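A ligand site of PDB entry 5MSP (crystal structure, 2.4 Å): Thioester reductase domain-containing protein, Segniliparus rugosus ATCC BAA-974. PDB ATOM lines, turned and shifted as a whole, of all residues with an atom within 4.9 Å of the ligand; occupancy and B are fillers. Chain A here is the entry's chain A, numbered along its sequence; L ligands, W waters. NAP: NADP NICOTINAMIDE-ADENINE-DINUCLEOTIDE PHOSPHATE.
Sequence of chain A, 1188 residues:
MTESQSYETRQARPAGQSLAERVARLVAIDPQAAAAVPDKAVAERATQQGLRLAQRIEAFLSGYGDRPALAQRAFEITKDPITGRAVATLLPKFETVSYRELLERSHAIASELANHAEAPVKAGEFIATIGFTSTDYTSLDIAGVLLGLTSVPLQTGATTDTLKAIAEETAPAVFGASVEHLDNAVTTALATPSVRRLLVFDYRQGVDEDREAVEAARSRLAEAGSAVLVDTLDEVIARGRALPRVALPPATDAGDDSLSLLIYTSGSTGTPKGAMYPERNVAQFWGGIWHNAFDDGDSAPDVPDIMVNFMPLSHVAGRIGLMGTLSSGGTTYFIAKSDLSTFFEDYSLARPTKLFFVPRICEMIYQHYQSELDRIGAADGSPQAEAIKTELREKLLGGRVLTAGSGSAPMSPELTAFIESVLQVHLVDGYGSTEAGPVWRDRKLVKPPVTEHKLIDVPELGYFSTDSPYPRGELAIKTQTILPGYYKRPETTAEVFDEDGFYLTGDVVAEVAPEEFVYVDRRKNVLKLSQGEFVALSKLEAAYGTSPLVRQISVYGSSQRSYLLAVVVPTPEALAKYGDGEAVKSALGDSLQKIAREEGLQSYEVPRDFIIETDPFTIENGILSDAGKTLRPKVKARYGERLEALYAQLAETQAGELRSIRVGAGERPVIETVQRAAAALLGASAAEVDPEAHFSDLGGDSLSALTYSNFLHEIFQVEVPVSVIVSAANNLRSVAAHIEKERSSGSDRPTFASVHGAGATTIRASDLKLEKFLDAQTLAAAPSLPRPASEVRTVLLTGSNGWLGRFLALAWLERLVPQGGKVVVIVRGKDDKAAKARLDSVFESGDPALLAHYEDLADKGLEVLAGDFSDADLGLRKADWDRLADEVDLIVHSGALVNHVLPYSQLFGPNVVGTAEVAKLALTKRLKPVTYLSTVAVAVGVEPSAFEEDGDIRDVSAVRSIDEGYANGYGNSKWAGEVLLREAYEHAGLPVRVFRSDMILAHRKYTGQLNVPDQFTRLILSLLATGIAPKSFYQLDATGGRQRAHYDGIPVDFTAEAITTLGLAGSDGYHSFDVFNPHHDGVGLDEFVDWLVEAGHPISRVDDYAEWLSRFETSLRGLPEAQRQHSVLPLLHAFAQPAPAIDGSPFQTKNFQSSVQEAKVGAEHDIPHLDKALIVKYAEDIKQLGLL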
ATOM      1  N   GLY A 799     -21.260   3.399   8.818  1.00  0.00           N
ATOM      2  CA  GLY A 799     -22.633   3.893   8.953  1.00  0.00           C
ATOM      3  C   GLY A 799     -22.763   5.256   9.584  1.00  0.00           C
ATOM      4  O   GLY A 799     -23.838   5.575  10.107  1.00  0.00           O
ATOM      5  N   SER A 800     -21.687   6.063   9.548  1.00  0.00           N
ATOM      6  CA  SER A 800     -21.704   7.349  10.195  1.00  0.00           C
ATOM      7  C   SER A 800     -22.685   8.385   9.659  1.00  0.00           C
ATOM      8  O   SER A 800     -22.980   9.299  10.372  1.00  0.00           O
ATOM      9  CB  SER A 800     -20.335   7.948  10.190  1.00  0.00           C
ATOM     10  OG  SER A 800     -19.907   8.066   8.886  1.00  0.00           O
ATOM     11  N   ASN A 801     -23.175   8.261   8.422  1.00  0.00           N
ATOM     12  CA  ASN A 801     -24.240   9.144   7.969  1.00  0.00           C
ATOM     13  C   ASN A 801     -25.620   8.584   8.274  1.00  0.00           C
ATOM     14  O   ASN A 801     -26.623   9.258   8.057  1.00  0.00           O
ATOM     15  CB  ASN A 801     -24.106   9.498   6.497  1.00  0.00           C
ATOM     16  CG  ASN A 801     -24.173   8.285   5.565  1.00  0.00           C
ATOM     17  OD1 ASN A 801     -23.366   7.353   5.646  1.00  0.00           O
ATOM     18  ND2 ASN A 801     -25.120   8.309   4.663  1.00  0.00           N
ATOM     19  N   GLY A 802     -25.657   7.379   8.844  1.00  0.00           N
ATOM     20  CA  GLY A 802     -26.914   6.801   9.339  1.00  0.00           C
ATOM     21  C   GLY A 802     -27.442   7.561  10.526  1.00  0.00           C
ATOM     22  O   GLY A 802     -26.795   8.495  11.050  1.00  0.00           O
ATOM     23  N   TRP A 803     -28.593   7.123  10.988  1.00  0.00           N
ATOM     24  CA  TRP A 803     -29.247   7.805  12.104  1.00  0.00           C
ATOM     25  C   TRP A 803     -28.512   7.601  13.439  1.00  0.00           C
ATOM     26  O   TRP A 803     -28.207   8.538  14.088  1.00  0.00           O
ATOM     27  CB  TRP A 803     -30.683   7.349  12.224  1.00  0.00           C
ATOM     28  CG  TRP A 803     -31.339   7.700  13.485  1.00  0.00           C
ATOM     29  CD1 TRP A 803     -31.915   6.845  14.355  1.00  0.00           C
ATOM     30  CD2 TRP A 803     -31.492   8.991  14.015  1.00  0.00           C
ATOM     31  NE1 TRP A 803     -32.429   7.524  15.379  1.00  0.00           N
ATOM     32  CE2 TRP A 803     -32.186   8.854  15.207  1.00  0.00           C
ATOM     33  CE3 TRP A 803     -31.104  10.250  13.600  1.00  0.00           C
ATOM     34  CZ2 TRP A 803     -32.496   9.925  16.018  1.00  0.00           C
ATOM     35  CZ3 TRP A 803     -31.438  11.319  14.372  1.00  0.00           C
ATOM     36  CH2 TRP A 803     -32.098  11.165  15.598  1.00  0.00           C
ATOM     37  N   LEU A 804     -28.261   6.370  13.804  1.00  0.00           N
ATOM     38  CA  LEU A 804     -27.479   6.066  14.993  1.00  0.00           C
ATOM     39  C   LEU A 804     -26.010   6.432  14.809  1.00  0.00           C
ATOM     40  O   LEU A 804     -25.385   7.028  15.679  1.00  0.00           O
ATOM     41  CB  LEU A 804     -27.642   4.593  15.416  1.00  0.00           C
ATOM     42  CG  LEU A 804     -26.831   4.136  16.623  1.00  0.00           C
ATOM     43  CD1 LEU A 804     -27.126   4.976  17.860  1.00  0.00           C
ATOM     44  CD2 LEU A 804     -27.072   2.681  16.882  1.00  0.00           C
ATOM     45  N   GLY A 805     -25.468   6.070  13.662  1.00  0.00           N
ATOM     46  CA  GLY A 805     -24.058   6.220  13.391  1.00  0.00           C
ATOM     47  C   GLY A 805     -23.523   7.627  13.539  1.00  0.00           C
ATOM     48  O   GLY A 805     -22.415   7.806  13.916  1.00  0.00           O
ATOM     49  N   ARG A 828     -20.439   6.029   1.807  1.00  0.00           N
ATOM     50  CA  ARG A 828     -20.604   5.818   0.379  1.00  0.00           C
ATOM     51  C   ARG A 828     -20.641   7.144  -0.376  1.00  0.00           C
ATOM     52  O   ARG A 828     -21.363   8.052   0.021  1.00  0.00           O
ATOM     53  CB  ARG A 828     -21.844   4.978   0.083  1.00  0.00           C
ATOM     54  CG  ARG A 828     -21.738   3.568   0.608  1.00  0.00           C
ATOM     55  CD  ARG A 828     -22.627   2.581  -0.091  1.00  0.00           C
ATOM     56  NE  ARG A 828     -24.015   2.762   0.282  1.00  0.00           N
ATOM     57  CZ  ARG A 828     -25.013   1.977  -0.125  1.00  0.00           C
ATOM     58  NH1 ARG A 828     -24.821   0.972  -0.980  1.00  0.00           N
ATOM     59  NH2 ARG A 828     -26.224   2.242   0.291  1.00  0.00           N
ATOM     60  N   ARG A 838     -21.703  14.292   2.057  1.00  0.00           N
ATOM     61  CA  ARG A 838     -22.867  13.546   2.490  1.00  0.00           C
ATOM     62  C   ARG A 838     -22.915  13.502   4.009  1.00  0.00           C
ATOM     63  O   ARG A 838     -23.977  13.740   4.596  1.00  0.00           O
ATOM     64  CB  ARG A 838     -22.857  12.118   1.972  1.00  0.00           C
ATOM     65  CG  ARG A 838     -23.024  11.998   0.478  1.00  0.00           C
ATOM     66  CD  ARG A 838     -23.245  10.556   0.089  1.00  0.00           C
ATOM     67  NE  ARG A 838     -24.564  10.095   0.503  1.00  0.00           N
ATOM     68  CZ  ARG A 838     -24.831   8.892   1.008  1.00  0.00           C
ATOM     69  NH1 ARG A 838     -23.876   7.944   1.196  1.00  0.00           N
ATOM     70  NH2 ARG A 838     -26.075   8.632   1.346  1.00  0.00           N
ATOM     71  N   GLY A 867     -16.170   4.624   0.444  1.00  0.00           N
ATOM     72  CA  GLY A 867     -16.072   3.187   0.391  1.00  0.00           C
ATOM     73  C   GLY A 867     -17.384   2.488   0.419  1.00  0.00           C
ATOM     74  O   GLY A 867     -18.452   3.102   0.362  1.00  0.00           O
ATOM     75  N   ASP A 868     -17.266   1.185   0.521  1.00  0.00           N
ATOM     76  CA  ASP A 868     -18.411   0.318   0.504  1.00  0.00           C
ATOM     77  C   ASP A 868     -17.969  -0.971   1.150  1.00  0.00           C
ATOM     78  O   ASP A 868     -17.144  -1.704   0.608  1.00  0.00           O
ATOM     79  CB  ASP A 868     -18.873   0.115  -0.937  1.00  0.00           C
ATOM     80  CG  ASP A 868     -20.210  -0.541  -1.033  1.00  0.00           C
ATOM     81  OD1 ASP A 868     -20.411  -1.561  -0.293  1.00  0.00           O
ATOM     82  OD2 ASP A 868     -21.055  -0.039  -1.864  1.00  0.00           O
ATOM     83  N   PHE A 869     -18.491  -1.265   2.326  1.00  0.00           N
ATOM     84  CA  PHE A 869     -18.066  -2.506   2.992  1.00  0.00           C
ATOM     85  C   PHE A 869     -18.521  -3.830   2.302  1.00  0.00           C
ATOM     86  O   PHE A 869     -17.963  -4.872   2.598  1.00  0.00           O
ATOM     87  CB  PHE A 869     -18.338  -2.483   4.505  1.00  0.00           C
ATOM     88  CG  PHE A 869     -19.726  -2.097   4.865  1.00  0.00           C
ATOM     89  CD1 PHE A 869     -20.785  -2.943   4.573  1.00  0.00           C
ATOM     90  CD2 PHE A 869     -19.995  -0.884   5.509  1.00  0.00           C
ATOM     91  CE1 PHE A 869     -22.077  -2.611   4.925  1.00  0.00           C
ATOM     92  CE2 PHE A 869     -21.290  -0.561   5.850  1.00  0.00           C
ATOM     93  CZ  PHE A 869     -22.331  -1.424   5.558  1.00  0.00           C
ATOM     94  N   SER A 870     -19.468  -3.772   1.363  1.00  0.00           N
ATOM     95  CA  SER A 870     -19.814  -4.971   0.624  1.00  0.00           C
ATOM     96  C   SER A 870     -18.684  -5.391  -0.318  1.00  0.00           C
ATOM     97  O   SER A 870     -18.616  -6.556  -0.696  1.00  0.00           O
ATOM     98  CB  SER A 870     -21.140  -4.811  -0.104  1.00  0.00           C
ATOM     99  OG  SER A 870     -20.957  -4.114  -1.302  1.00  0.00           O
ATOM    100  N   SER A 894     -21.746   0.059  12.392  1.00  0.00           N
ATOM    101  CA  SER A 894     -23.123   0.536  12.522  1.00  0.00           C
ATOM    102  C   SER A 894     -23.854   0.461  11.195  1.00  0.00           C
ATOM    103  O   SER A 894     -25.023   0.617  11.135  1.00  0.00           O
ATOM    104  CB  SER A 894     -23.126   1.982  12.957  1.00  0.00           C
ATOM    105  OG  SER A 894     -24.428   2.344  13.249  1.00  0.00           O
ATOM    106  N   GLY A 895     -23.148   0.182  10.132  1.00  0.00           N
ATOM    107  CA  GLY A 895     -23.767   0.201   8.828  1.00  0.00           C
ATOM    108  C   GLY A 895     -24.420  -1.102   8.436  1.00  0.00           C
ATOM    109  O   GLY A 895     -23.981  -2.173   8.824  1.00  0.00           O
ATOM    110  N   ALA A 896     -25.434  -0.959   7.621  1.00  0.00           N
ATOM    111  CA  ALA A 896     -26.230  -2.029   7.138  1.00  0.00           C
ATOM    112  C   ALA A 896     -27.271  -1.461   6.171  1.00  0.00           C
ATOM    113  O   ALA A 896     -27.547  -0.263   6.189  1.00  0.00           O
ATOM    114  CB  ALA A 896     -26.915  -2.711   8.314  1.00  0.00           C
ATOM    115  N   LEU A 897     -27.834  -2.339   5.333  1.00  0.00           N
ATOM    116  CA  LEU A 897     -29.043  -2.027   4.588  1.00  0.00           C
ATOM    117  C   LEU A 897     -30.213  -2.374   5.497  1.00  0.00           C
ATOM    118  O   LEU A 897     -30.549  -3.553   5.680  1.00  0.00           O
ATOM    119  CB  LEU A 897     -29.110  -2.778   3.277  1.00  0.00           C
ATOM    120  CG  LEU A 897     -30.264  -2.488   2.291  1.00  0.00           C
ATOM    121  CD1 LEU A 897     -30.684  -1.040   2.268  1.00  0.00           C
ATOM    122  CD2 LEU A 897     -29.874  -2.965   0.875  1.00  0.00           C
ATOM    123  N   VAL A 898     -30.835  -1.330   6.055  1.00  0.00           N
ATOM    124  CA  VAL A 898     -31.916  -1.460   7.060  1.00  0.00           C
ATOM    125  C   VAL A 898     -33.251  -1.272   6.330  1.00  0.00           C
ATOM    126  O   VAL A 898     -33.684  -0.147   6.064  1.00  0.00           O
ATOM    127  CB  VAL A 898     -31.799  -0.452   8.246  1.00  0.00           C
ATOM    128  CG1 VAL A 898     -32.874  -0.710   9.292  1.00  0.00           C
ATOM    129  CG2 VAL A 898     -30.447  -0.493   8.886  1.00  0.00           C
ATOM    130  N   PRO A 910     -24.715  -6.430   1.658  1.00  0.00           N
ATOM    131  CA  PRO A 910     -24.437  -5.417   2.674  1.00  0.00           C
ATOM    132  C   PRO A 910     -24.328  -5.953   4.103  1.00  0.00           C
ATOM    133  O   PRO A 910     -23.406  -5.604   4.840  1.00  0.00           O
ATOM    134  CB  PRO A 910     -25.626  -4.458   2.567  1.00  0.00           C
ATOM    135  CG  PRO A 910     -26.611  -5.110   1.659  1.00  0.00           C
ATOM    136  CD  PRO A 910     -25.879  -6.096   0.826  1.00  0.00           C
ATOM    137  N   LEU A 933     -23.763  -3.501  15.525  1.00  0.00           N
ATOM    138  CA  LEU A 933     -25.143  -3.120  15.774  1.00  0.00           C
ATOM    139  C   LEU A 933     -26.014  -4.163  15.137  1.00  0.00           C
ATOM    140  O   LEU A 933     -25.717  -4.586  14.048  1.00  0.00           O
ATOM    141  CB  LEU A 933     -25.455  -1.766  15.200  1.00  0.00           C
ATOM    142  CG  LEU A 933     -25.113  -0.587  16.097  1.00  0.00           C
ATOM    143  CD1 LEU A 933     -26.107  -0.477  17.209  1.00  0.00           C
ATOM    144  CD2 LEU A 933     -23.712  -0.672  16.639  1.00  0.00           C
ATOM    145  N   SER A 934     -27.017  -4.621  15.869  1.00  0.00           N
ATOM    146  CA  SER A 934     -27.903  -5.644  15.388  1.00  0.00           C
ATOM    147  C   SER A 934     -29.313  -5.273  15.833  1.00  0.00           C
ATOM    148  O   SER A 934     -29.567  -4.091  16.066  1.00  0.00           O
ATOM    149  CB  SER A 934     -27.427  -7.011  15.818  1.00  0.00           C
ATOM    150  OG  SER A 934     -28.208  -8.054  15.232  1.00  0.00           O
ATOM    151  N   THR A 935     -30.216  -6.247  15.918  1.00  0.00           N
ATOM    152  CA  THR A 935     -31.667  -6.006  16.041  1.00  0.00           C
ATOM    153  C   THR A 935     -32.352  -7.195  16.710  1.00  0.00           C
ATOM    154  O   THR A 935     -31.891  -8.318  16.666  1.00  0.00           O
ATOM    155  CB  THR A 935     -32.316  -5.766  14.644  1.00  0.00           C
ATOM    156  OG1 THR A 935     -33.715  -5.808  14.735  1.00  0.00           O
ATOM    157  CG2 THR A 935     -31.964  -6.843  13.685  1.00  0.00           C
ATOM    158  N   TYR A 970     -34.480  -8.918   6.660  1.00  0.00           N
ATOM    159  CA  TYR A 970     -33.691  -8.081   7.549  1.00  0.00           C
ATOM    160  C   TYR A 970     -33.124  -8.867   8.757  1.00  0.00           C
ATOM    161  O   TYR A 970     -31.884  -8.965   8.928  1.00  0.00           O
ATOM    162  CB  TYR A 970     -34.492  -6.888   8.019  1.00  0.00           C
ATOM    163  CG  TYR A 970     -33.751  -5.952   8.932  1.00  0.00           C
ATOM    164  CD1 TYR A 970     -34.282  -5.590  10.143  1.00  0.00           C
ATOM    165  CD2 TYR A 970     -32.484  -5.486   8.603  1.00  0.00           C
ATOM    166  CE1 TYR A 970     -33.617  -4.740  10.987  1.00  0.00           C
ATOM    167  CE2 TYR A 970     -31.805  -4.611   9.433  1.00  0.00           C
ATOM    168  CZ  TYR A 970     -32.378  -4.233  10.622  1.00  0.00           C
ATOM    169  OH  TYR A 970     -31.718  -3.383  11.496  1.00  0.00           O
ATOM    170  N   LYS A 974     -29.163  -9.774   9.552  1.00  0.00           N
ATOM    171  CA  LYS A 974     -28.465  -9.311  10.760  1.00  0.00           C
ATOM    172  C   LYS A 974     -27.943 -10.495  11.617  1.00  0.00           C
ATOM    173  O   LYS A 974     -26.831 -10.440  12.099  1.00  0.00           O
ATOM    174  CB  LYS A 974     -29.329  -8.350  11.564  1.00  0.00           C
ATOM    175  CG  LYS A 974     -29.621  -7.030  10.834  1.00  0.00           C
ATOM    176  CD  LYS A 974     -28.381  -6.216  10.418  1.00  0.00           C
ATOM    177  CE  LYS A 974     -27.482  -5.815  11.588  1.00  0.00           C
ATOM    178  NZ  LYS A 974     -26.329  -4.990  11.148  1.00  0.00           N
ATOM    179  N   SER A 997     -30.735  -3.143  18.760  1.00  0.00           N
ATOM    180  CA  SER A 997     -31.476  -1.966  19.059  1.00  0.00           C
ATOM    181  C   SER A 997     -32.455  -1.689  18.009  1.00  0.00           C
ATOM    182  O   SER A 997     -32.072  -1.716  16.820  1.00  0.00           O
ATOM    183  CB  SER A 997     -30.537  -0.800  19.151  1.00  0.00           C
ATOM    184  OG  SER A 997     -30.200  -0.292  17.883  1.00  0.00           O
ATOM    185  N   ASN A1011     -35.061  10.300  13.334  1.00  0.00           N
ATOM    186  CA  ASN A1011     -35.041   9.430  12.167  1.00  0.00           C
ATOM    187  C   ASN A1011     -36.330   9.606  11.388  1.00  0.00           C
ATOM    188  O   ASN A1011     -37.333   9.067  11.802  1.00  0.00           O
ATOM    189  CB  ASN A1011     -34.924   7.983  12.654  1.00  0.00           C
ATOM    190  CG  ASN A1011     -34.466   7.034  11.589  1.00  0.00           C
ATOM    191  OD1 ASN A1011     -34.220   7.406  10.467  1.00  0.00           O
ATOM    192  ND2 ASN A1011     -34.318   5.796  11.967  1.00  0.00           N
HETATM  193  PA  NAP L   1     -29.550   3.781   8.820  1.00  0.00           P
HETATM  194  O1A NAP L   1     -30.062   5.109   9.280  1.00  0.00           O
HETATM  195  O2A NAP L   1     -30.296   3.139   7.689  1.00  0.00           O
HETATM  196  O5B NAP L   1     -27.992   3.902   8.459  1.00  0.00           O
HETATM  197  C5B NAP L   1     -27.341   2.937   7.648  1.00  0.00           C
HETATM  198  C4B NAP L   1     -25.915   3.374   7.293  1.00  0.00           C
HETATM  199  O4B NAP L   1     -25.162   2.359   6.600  1.00  0.00           O
HETATM  200  C3B NAP L   1     -25.854   4.571   6.384  1.00  0.00           C
HETATM  201  O3B NAP L   1     -24.699   5.312   6.778  1.00  0.00           O
HETATM  202  C2B NAP L   1     -25.672   3.956   5.008  1.00  0.00           C
HETATM  203  O2B NAP L   1     -25.030   4.747   4.005  1.00  0.00           O
HETATM  204  C1B NAP L   1     -24.708   2.889   5.368  1.00  0.00           C
HETATM  205  N9A NAP L   1     -24.620   1.808   4.406  1.00  0.00           N
HETATM  206  C8A NAP L   1     -25.616   1.048   3.921  1.00  0.00           C
HETATM  207  N7A NAP L   1     -25.086   0.159   3.106  1.00  0.00           N
HETATM  208  C5A NAP L   1     -23.778   0.353   3.043  1.00  0.00           C
HETATM  209  C6A NAP L   1     -22.626  -0.229   2.335  1.00  0.00           C
HETATM  210  N6A NAP L   1     -22.777  -1.269   1.486  1.00  0.00           N
HETATM  211  N1A NAP L   1     -21.386   0.303   2.560  1.00  0.00           N
HETATM  212  C2A NAP L   1     -21.224   1.364   3.360  1.00  0.00           C
HETATM  213  N3A NAP L   1     -22.234   1.942   4.035  1.00  0.00           N
HETATM  214  C4A NAP L   1     -23.478   1.459   3.910  1.00  0.00           C
HETATM  215  O3  NAP L   1     -29.539   2.733   9.988  1.00  0.00           O
HETATM  216  PN  NAP L   1     -29.409   3.187  11.542  1.00  0.00           P
HETATM  217  O1N NAP L   1     -30.793   3.578  11.954  1.00  0.00           O
HETATM  218  O2N NAP L   1     -28.258   4.082  11.834  1.00  0.00           O
HETATM  219  O5D NAP L   1     -29.133   1.753  12.080  1.00  0.00           O
HETATM  220  C5D NAP L   1     -27.951   1.465  12.755  1.00  0.00           C
HETATM  221  C4D NAP L   1     -27.913   0.018  13.132  1.00  0.00           C
HETATM  222  O4D NAP L   1     -28.969  -0.387  14.003  1.00  0.00           O
HETATM  223  C3D NAP L   1     -27.979  -0.831  11.893  1.00  0.00           C
HETATM  224  O3D NAP L   1     -26.872  -1.649  11.715  1.00  0.00           O
HETATM  225  C2D NAP L   1     -29.115  -1.726  12.181  1.00  0.00           C
HETATM  226  O2D NAP L   1     -28.940  -2.954  11.499  1.00  0.00           O
HETATM  227  C1D NAP L   1     -29.160  -1.756  13.687  1.00  0.00           C
HETATM  228  N1N NAP L   1     -30.483  -2.110  14.068  1.00  0.00           N
HETATM  229  P2B NAP L   1     -25.889   5.170   2.735  1.00  0.00           P
HETATM  230  O1X NAP L   1     -26.892   4.083   2.565  1.00  0.00           O
HETATM  231  O2X NAP L   1     -26.515   6.398   3.178  1.00  0.00           O
HETATM  232  O3X NAP L   1     -24.846   5.160   1.670  1.00  0.00           O
HETATM  233  O   HOH W   1     -30.215   1.467   5.653  1.00  0.00           O
HETATM  234  O   HOH W   2     -25.705   3.764  11.375  1.00  0.00           O
HETATM  235  O   HOH W   3     -32.957   3.788   8.267  1.00  0.00           O
HETATM  236  O   HOH W   4     -26.150   5.696  -0.699  1.00  0.00           O
HETATM  237  O   HOH W   5     -26.543  -1.277   0.833  1.00  0.00           O
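The side-chain amide oxygen of Asn 801 is in hydrogen-bond range of an oxygen (O3B) of the ligand, at 2.7 Å.
The side-chain hydroxyl (OH) of Tyr 970 is in hydrogen-bond range of an oxygen (O2D) of the ligand, 2.8 Å away.
The guanidinium group of Arg 828 is in salt-bridge range of an oxygen (O3X) of the ligand, at 2.9 Å.
An oxygen (O2X) of the ligand is in salt-bridge range of the guanidinium group (NH2) of Arg 838 (2.9 Å).
A nitrogen (N6A) of the ligand is in hydrogen-bond range of the side-chain carboxylate (OD1) of Asp 868.
O of Ser 894 is in hydrogen-bond range of O3D of the ligand.
N of Leu 804 is in hydrogen-bond range of O2N of the ligand (3.0 Å).
N of Trp 803 is in hydrogen-bond range of O1A of the ligand, at 3.0 Å.
The backbone NH of Gly 802 sits at hydrogen-bond distance from an oxygen (O3B) of the ligand, at 3.1 Å.
The backbone NH (N) of Phe 869 sits at hydrogen-bond distance from a nitrogen (N1A) of the ligand, 3.3 Å away.
NZ of Lys 974 lies close to O2D of the ligand (3.3 Å).
The backbone NH (N) of Ala 896 lies within hydrogen-bond range of an oxygen (O4B) of the ligand (3.5 Å).
The backbone carbonyl oxygen (O) of Gly 799 lies close to an oxygen (O3B) of the ligand, 3.4 Å away.
ND2 of Asn 801 sits close to NH2 of Arg 838.
NH1 of Arg 838 sits at hydrogen-bond distance from O of Arg 828 (2.8 Å).
The guanidinium group (NH1) of Arg 828 lies within salt-bridge range of the side-chain carboxylate (OD2) of Asp 868.
The backbone carbonyl oxygen of Ser 934 sits at hydrogen-bond distance from the backbone NH of Ser 997 (3.1 Å).
The side-chain hydroxyl (OG) of Ser 870 is in hydrogen-bond range of the side-chain carboxylate (OD1) of Asp 868.
The side-chain amino group (NZ) of Lys 974 is in hydrogen-bond range of the backbone carbonyl oxygen (O) of Leu 933 (3.0 Å).
O of Ser 934 sits close to N1N of the ligand, 3.0 Å away.
A nitrogen (N1N) of the ligand lies close to the backbone carbonyl oxygen of Ser 997 (3.2 Å).
N of Gly 805 touches O2N of the ligand, at 3.9 Å.
CA of Gly 895 touches O4B of the ligand, 3.4 Å away.
CG2 of Val 898 touches O3 of the ligand, at 3.5 Å.
Leu 933 touches the ligand (CB to C4D, 3.7 Å).
Hydrophobic or aromatic side chains that line the ligand: Trp 803, Leu 804, Phe 869, Ala 896, Val 898, Leu 933 and Tyr 970.
Within 4 Å of the ligand: Gly 799, Asn 801, Gly 802, Trp 803, Leu 804, Gly 805, Arg 828, Arg 838, Asp 868, Phe 869, Ser 894, Gly 895, Ala 896, Val 898, Leu 933, Ser 934, Tyr 970, Lys 974 and Ser 997.
Water W2 lies within hydrogen-bond range of O2N of the ligand (2.6 Å), OG of Ser 894 (2.7 Å), O of Gly 799 (2.9 Å) and N of Gly 805 (3.3 Å).
Water W1 lies within hydrogen-bond range of O2A of the ligand (2.6 Å), N of Val 898 (2.9 Å) and O of Ala 896 (3.2 Å).
Water W5 bridges N7A of the ligand (3.1 Å) and NH1 of Arg 828 (3.4 Å).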
